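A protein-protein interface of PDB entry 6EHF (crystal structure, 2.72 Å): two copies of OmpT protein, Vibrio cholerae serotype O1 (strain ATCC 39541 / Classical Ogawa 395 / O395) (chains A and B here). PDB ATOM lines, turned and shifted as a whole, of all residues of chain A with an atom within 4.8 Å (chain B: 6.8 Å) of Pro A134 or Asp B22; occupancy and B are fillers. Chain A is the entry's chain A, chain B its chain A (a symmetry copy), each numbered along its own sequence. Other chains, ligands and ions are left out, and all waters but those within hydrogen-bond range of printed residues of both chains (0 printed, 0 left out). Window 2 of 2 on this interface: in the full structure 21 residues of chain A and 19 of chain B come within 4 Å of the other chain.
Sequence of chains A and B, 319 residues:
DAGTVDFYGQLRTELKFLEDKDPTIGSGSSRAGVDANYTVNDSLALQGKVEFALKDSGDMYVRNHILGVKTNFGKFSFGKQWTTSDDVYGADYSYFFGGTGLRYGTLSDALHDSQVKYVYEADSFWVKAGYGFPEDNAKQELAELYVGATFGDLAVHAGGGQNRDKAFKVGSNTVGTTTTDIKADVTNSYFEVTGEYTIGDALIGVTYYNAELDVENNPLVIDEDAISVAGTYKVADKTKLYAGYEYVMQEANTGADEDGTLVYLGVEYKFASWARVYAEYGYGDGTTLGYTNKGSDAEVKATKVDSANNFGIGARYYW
The side-chain carboxylate (OD1) of Asp A136 is in hydrogen-bond range of the backbone NH (N) of Asp B22, 3.0 Å away.
Among the printed residues, merely in contact across the chains: Phe A133 with Pro B23 (3.5 Å), Glu A135 with Thr B24 (3.7 Å), Glu A135 with Pro B23 (3.8 Å), Asp A136 with Lys B21 (3.9 Å) and Pro A134 with Asp B22 (3.9 Å).
The backbone carbonyl oxygen (O) of Pro A134 lies within hydrogen-bond range of the backbone NH (N) of Lys A139. O of Lys B16 sits at hydrogen-bond distance from N of Thr B24 (3.1 Å).
Of the printed residues of chain B, Phe A133 touches Pro B23 (3.5 Å). Of chain B, only Asp B22 comes within 4 Å of Pro A134. Of the printed residues of chain B, Asp A136 touches Lys B21 and Asp B22. Lys A139 touches none of the printed residues of chain B. Gln A140 touches none of the printed residues of chain B. Of chain A, only Pro A134 (3.9 Å) and Asp A136 (3.0 Å) come within 4 Å of Asp B22. Of the printed residues of chain A, Pro B23 touches Phe A133 (3.5 Å) and Glu A135 (3.8 Å). Printed residues of chain A within 4 Å of Thr B24: Glu A135. The nearest residue of chain B that does not touch Pro A134 is Pro B23 (5.4 Å). The nearest printed residue of chain A that does not touch Thr B24 is Phe A133 (4.3 Å).
Hydrophobic or aromatic side chains of chain B that line the printed part of chain A: Pro B23. Along chain A the printed residues that touch a printed residue of chain B span positions 133 to 136. Among the printed residues, 6 pairs touch across the chains.
No position is printed for both chains.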
ATOM      1  N   TYR A 131      18.682  18.026   2.835  1.00  0.00           N
ATOM      2  CA  TYR A 131      19.529  16.999   3.396  1.00  0.00           C
ATOM      3  C   TYR A 131      19.996  17.477   4.783  1.00  0.00           C
ATOM      4  O   TYR A 131      20.416  18.631   4.932  1.00  0.00           O
ATOM      5  CB  TYR A 131      20.717  16.722   2.433  1.00  0.00           C
ATOM      6  CG  TYR A 131      21.839  15.899   3.026  1.00  0.00           C
ATOM      7  CD1 TYR A 131      21.775  14.528   3.071  1.00  0.00           C
ATOM      8  CD2 TYR A 131      22.959  16.504   3.556  1.00  0.00           C
ATOM      9  CE1 TYR A 131      22.812  13.767   3.614  1.00  0.00           C
ATOM     10  CE2 TYR A 131      23.993  15.749   4.117  1.00  0.00           C
ATOM     11  CZ  TYR A 131      23.927  14.387   4.144  1.00  0.00           C
ATOM     12  OH  TYR A 131      24.977  13.683   4.732  1.00  0.00           O
ATOM     13  N   GLY A 132      19.923  16.572   5.767  1.00  0.00           N
ATOM     14  CA  GLY A 132      20.478  16.750   7.133  1.00  0.00           C
ATOM     15  C   GLY A 132      21.821  16.046   7.308  1.00  0.00           C
ATOM     16  O   GLY A 132      21.964  14.841   7.081  1.00  0.00           O
ATOM     17  N   PHE A 133      22.810  16.827   7.692  1.00  0.00           N
ATOM     18  CA  PHE A 133      24.135  16.335   7.967  1.00  0.00           C
ATOM     19  C   PHE A 133      24.080  15.720   9.336  1.00  0.00           C
ATOM     20  O   PHE A 133      23.779  16.404  10.324  1.00  0.00           O
ATOM     21  CB  PHE A 133      25.145  17.478   8.084  1.00  0.00           C
ATOM     22  CG  PHE A 133      25.633  18.042   6.771  1.00  0.00           C
ATOM     23  CD1 PHE A 133      24.752  18.366   5.733  1.00  0.00           C
ATOM     24  CD2 PHE A 133      26.992  18.320   6.602  1.00  0.00           C
ATOM     25  CE1 PHE A 133      25.238  18.889   4.543  1.00  0.00           C
ATOM     26  CE2 PHE A 133      27.469  18.862   5.426  1.00  0.00           C
ATOM     27  CZ  PHE A 133      26.598  19.146   4.395  1.00  0.00           C
ATOM     28  N   PRO A 134      24.425  14.446   9.435  1.00  0.00           N
ATOM     29  CA  PRO A 134      24.437  13.862  10.760  1.00  0.00           C
ATOM     30  C   PRO A 134      25.517  14.385  11.694  1.00  0.00           C
ATOM     31  O   PRO A 134      25.444  14.011  12.848  1.00  0.00           O
ATOM     32  CB  PRO A 134      24.653  12.399  10.473  1.00  0.00           C
ATOM     33  CG  PRO A 134      25.432  12.393   9.232  1.00  0.00           C
ATOM     34  CD  PRO A 134      24.825  13.475   8.409  1.00  0.00           C
ATOM     35  N   GLU A 135      26.474  15.228  11.233  1.00  0.00           N
ATOM     36  CA  GLU A 135      27.484  15.905  12.111  1.00  0.00           C
ATOM     37  C   GLU A 135      27.866  14.756  13.182  1.00  0.00           C
ATOM     38  O   GLU A 135      27.600  14.877  14.396  1.00  0.00           O
ATOM     39  CB  GLU A 135      27.000  17.367  12.730  1.00  0.00           C
ATOM     40  CG  GLU A 135      26.677  18.763  11.944  1.00  0.00           C
ATOM     41  CD  GLU A 135      26.470  20.078  12.904  1.00  0.00           C
ATOM     42  OE1 GLU A 135      26.257  21.332  12.588  1.00  0.00           O
ATOM     43  OE2 GLU A 135      26.515  19.884  14.137  1.00  0.00           O
ATOM     44  N   ASP A 136      28.396  13.612  12.694  1.00  0.00           N
ATOM     45  CA  ASP A 136      28.748  12.355  13.505  1.00  0.00           C
ATOM     46  C   ASP A 136      27.775  11.800  14.551  1.00  0.00           C
ATOM     47  O   ASP A 136      28.154  11.509  15.695  1.00  0.00           O
ATOM     48  CB  ASP A 136      30.089  12.469  14.224  1.00  0.00           C
ATOM     49  CG  ASP A 136      31.201  12.676  13.296  1.00  0.00           C
ATOM     50  OD1 ASP A 136      31.263  13.782  12.712  1.00  0.00           O
ATOM     51  OD2 ASP A 136      32.020  11.749  13.154  1.00  0.00           O
ATOM     52  N   ASN A 137      26.526  11.628  14.154  1.00  0.00           N
ATOM     53  CA  ASN A 137      25.469  11.083  15.027  1.00  0.00           C
ATOM     54  C   ASN A 137      25.058  11.886  16.248  1.00  0.00           C
ATOM     55  O   ASN A 137      24.167  11.480  16.980  1.00  0.00           O
ATOM     56  CB  ASN A 137      25.788   9.653  15.407  1.00  0.00           C
ATOM     57  CG  ASN A 137      25.843   8.772  14.200  1.00  0.00           C
ATOM     58  OD1 ASN A 137      25.095   8.970  13.208  1.00  0.00           O
ATOM     59  ND2 ASN A 137      26.746   7.810  14.246  1.00  0.00           N
ATOM     60  N   ALA A 138      25.664  13.049  16.429  1.00  0.00           N
ATOM     61  CA  ALA A 138      25.059  14.099  17.211  1.00  0.00           C
ATOM     62  C   ALA A 138      23.719  14.559  16.639  1.00  0.00           C
ATOM     63  O   ALA A 138      22.950  15.185  17.379  1.00  0.00           O
ATOM     64  CB  ALA A 138      25.994  15.273  17.295  1.00  0.00           C
ATOM     65  N   LYS A 139      23.454  14.298  15.346  1.00  0.00           N
ATOM     66  CA  LYS A 139      22.169  14.636  14.735  1.00  0.00           C
ATOM     67  C   LYS A 139      21.623  13.515  13.915  1.00  0.00           C
ATOM     68  O   LYS A 139      22.392  12.649  13.422  1.00  0.00           O
ATOM     69  CB  LYS A 139      22.285  15.822  13.780  1.00  0.00           C
ATOM     70  CG  LYS A 139      23.251  16.904  14.185  1.00  0.00           C
ATOM     71  CD  LYS A 139      22.725  17.754  15.315  1.00  0.00           C
ATOM     72  CE  LYS A 139      23.816  18.689  15.808  1.00  0.00           C
ATOM     73  NZ  LYS A 139      23.347  19.359  17.031  1.00  0.00           N
ATOM     74  N   GLN A 140      20.305  13.606  13.709  1.00  0.00           N
ATOM     75  CA  GLN A 140      19.563  12.664  12.848  1.00  0.00           C
ATOM     76  C   GLN A 140      20.017  12.678  11.386  1.00  0.00           C
ATOM     77  O   GLN A 140      20.408  13.701  10.878  1.00  0.00           O
ATOM     78  CB  GLN A 140      18.046  12.959  12.890  1.00  0.00           C
ATOM     79  CG  GLN A 140      17.446  12.764  14.274  1.00  0.00           C
ATOM     80  CD  GLN A 140      15.989  13.126  14.406  1.00  0.00           C
ATOM     81  OE1 GLN A 140      15.428  13.908  13.631  1.00  0.00           O
ATOM     82  NE2 GLN A 140      15.363  12.561  15.428  1.00  0.00           N
ATOM     83  N   GLU A 141      19.968  11.523  10.733  1.00  0.00           N
ATOM     84  CA  GLU A 141      20.007  11.432   9.265  1.00  0.00           C
ATOM     85  C   GLU A 141      18.659  11.895   8.751  1.00  0.00           C
ATOM     86  O   GLU A 141      17.621  11.450   9.277  1.00  0.00           O
ATOM     87  CB  GLU A 141      20.188   9.999   8.781  1.00  0.00           C
ATOM     88  CG  GLU A 141      21.619   9.549   8.551  1.00  0.00           C
ATOM     89  CD  GLU A 141      21.684   8.033   8.446  1.00  0.00           C
ATOM     90  OE1 GLU A 141      20.876   7.435   7.693  1.00  0.00           O
ATOM     91  OE2 GLU A 141      22.506   7.432   9.152  1.00  0.00           O
ATOM     92  N   LYS B  16      32.668  22.784   7.706  1.00  0.00           N
ATOM     93  CA  LYS B  16      33.964  22.322   8.191  1.00  0.00           C
ATOM     94  C   LYS B  16      34.199  20.837   7.998  1.00  0.00           C
ATOM     95  O   LYS B  16      33.326  20.018   8.268  1.00  0.00           O
ATOM     96  CB  LYS B  16      34.124  22.662   9.676  1.00  0.00           C
ATOM     97  CG  LYS B  16      34.317  24.144   9.974  1.00  0.00           C
ATOM     98  CD  LYS B  16      34.043  24.519  11.430  1.00  0.00           C
ATOM     99  CE  LYS B  16      35.200  24.204  12.346  1.00  0.00           C
ATOM    100  NZ  LYS B  16      34.790  23.930  13.757  1.00  0.00           N
ATOM    101  N   PHE B  17      35.425  20.522   7.585  1.00  0.00           N
ATOM    102  CA  PHE B  17      35.896  19.170   7.351  1.00  0.00           C
ATOM    103  C   PHE B  17      37.139  18.953   8.231  1.00  0.00           C
ATOM    104  O   PHE B  17      38.231  19.389   7.873  1.00  0.00           O
ATOM    105  CB  PHE B  17      36.297  19.022   5.868  1.00  0.00           C
ATOM    106  CG  PHE B  17      35.193  19.298   4.883  1.00  0.00           C
ATOM    107  CD1 PHE B  17      34.893  20.596   4.496  1.00  0.00           C
ATOM    108  CD2 PHE B  17      34.493  18.264   4.303  1.00  0.00           C
ATOM    109  CE1 PHE B  17      33.890  20.863   3.561  1.00  0.00           C
ATOM    110  CE2 PHE B  17      33.482  18.515   3.375  1.00  0.00           C
ATOM    111  CZ  PHE B  17      33.172  19.820   3.007  1.00  0.00           C
ATOM    112  N   LEU B  18      37.001  18.302   9.380  1.00  0.00           N
ATOM    113  CA  LEU B  18      38.152  18.122  10.289  1.00  0.00           C
ATOM    114  C   LEU B  18      38.604  16.666  10.306  1.00  0.00           C
ATOM    115  O   LEU B  18      37.775  15.783  10.085  1.00  0.00           O
ATOM    116  CB  LEU B  18      37.774  18.576  11.695  1.00  0.00           C
ATOM    117  CG  LEU B  18      36.861  19.805  11.845  1.00  0.00           C
ATOM    118  CD1 LEU B  18      36.733  20.282  13.305  1.00  0.00           C
ATOM    119  CD2 LEU B  18      37.394  20.925  10.982  1.00  0.00           C
ATOM    120  N   GLU B  19      39.889  16.414  10.585  1.00  0.00           N
ATOM    121  CA  GLU B  19      40.472  15.048  10.451  1.00  0.00           C
ATOM    122  C   GLU B  19      39.615  14.027  11.234  1.00  0.00           C
ATOM    123  O   GLU B  19      39.138  14.317  12.317  1.00  0.00           O
ATOM    124  CB  GLU B  19      42.025  15.005  10.776  1.00  0.00           C
ATOM    125  CG  GLU B  19      42.754  13.648  11.064  1.00  0.00           C
ATOM    126  CD  GLU B  19      43.474  12.937   9.874  1.00  0.00           C
ATOM    127  OE1 GLU B  19      44.378  12.066  10.132  1.00  0.00           O
ATOM    128  OE2 GLU B  19      43.140  13.225   8.693  1.00  0.00           O
ATOM    129  N   ASP B  20      39.347  12.883  10.591  1.00  0.00           N
ATOM    130  CA  ASP B  20      38.700  11.699  11.185  1.00  0.00           C
ATOM    131  C   ASP B  20      37.180  11.825  11.486  1.00  0.00           C
ATOM    132  O   ASP B  20      36.564  10.848  11.980  1.00  0.00           O
ATOM    133  CB  ASP B  20      39.502  11.190  12.407  1.00  0.00           C
ATOM    134  CG  ASP B  20      40.968  10.787  12.065  1.00  0.00           C
ATOM    135  OD1 ASP B  20      41.362  10.646  10.861  1.00  0.00           O
ATOM    136  OD2 ASP B  20      41.734  10.595  13.040  1.00  0.00           O
ATOM    137  N   LYS B  21      36.590  12.973  11.102  1.00  0.00           N
ATOM    138  CA  LYS B  21      35.195  13.388  11.413  1.00  0.00           C
ATOM    139  C   LYS B  21      34.357  13.604  10.140  1.00  0.00           C
ATOM    140  O   LYS B  21      34.872  13.590   9.031  1.00  0.00           O
ATOM    141  CB  LYS B  21      35.174  14.717  12.198  1.00  0.00           C
ATOM    142  CG  LYS B  21      36.098  14.827  13.414  1.00  0.00           C
ATOM    143  CD  LYS B  21      35.571  14.107  14.647  1.00  0.00           C
ATOM    144  CE  LYS B  21      34.610  14.988  15.437  1.00  0.00           C
ATOM    145  NZ  LYS B  21      33.488  14.199  16.040  1.00  0.00           N
ATOM    146  N   ASP B  22      33.060  13.814  10.321  1.00  0.00           N
ATOM    147  CA  ASP B  22      32.137  14.104   9.228  1.00  0.00           C
ATOM    148  C   ASP B  22      32.080  15.601   9.005  1.00  0.00           C
ATOM    149  O   ASP B  22      32.447  16.380   9.885  1.00  0.00           O
ATOM    150  CB  ASP B  22      30.682  13.698   9.554  1.00  0.00           C
ATOM    151  CG  ASP B  22      30.463  12.213   9.638  1.00  0.00           C
ATOM    152  OD1 ASP B  22      31.444  11.442   9.617  1.00  0.00           O
ATOM    153  OD2 ASP B  22      29.276  11.840   9.741  1.00  0.00           O
ATOM    154  N   PRO B  23      31.564  16.006   7.843  1.00  0.00           N
ATOM    155  CA  PRO B  23      31.189  17.389   7.608  1.00  0.00           C
ATOM    156  C   PRO B  23      30.236  17.940   8.675  1.00  0.00           C
ATOM    157  O   PRO B  23      29.322  17.232   9.095  1.00  0.00           O
ATOM    158  CB  PRO B  23      30.469  17.332   6.244  1.00  0.00           C
ATOM    159  CG  PRO B  23      31.076  16.176   5.548  1.00  0.00           C
ATOM    160  CD  PRO B  23      31.464  15.195   6.612  1.00  0.00           C
ATOM    161  N   THR B  24      30.481  19.176   9.102  1.00  0.00           N
ATOM    162  CA  THR B  24      29.544  19.918   9.901  1.00  0.00           C
ATOM    163  C   THR B  24      29.054  21.100   9.087  1.00  0.00           C
ATOM    164  O   THR B  24      29.836  21.702   8.376  1.00  0.00           O
ATOM    165  CB  THR B  24      30.188  20.481  11.191  1.00  0.00           C
ATOM    166  OG1 THR B  24      31.022  21.601  10.863  1.00  0.00           O
ATOM    167  CG2 THR B  24      31.001  19.448  11.909  1.00  0.00           C
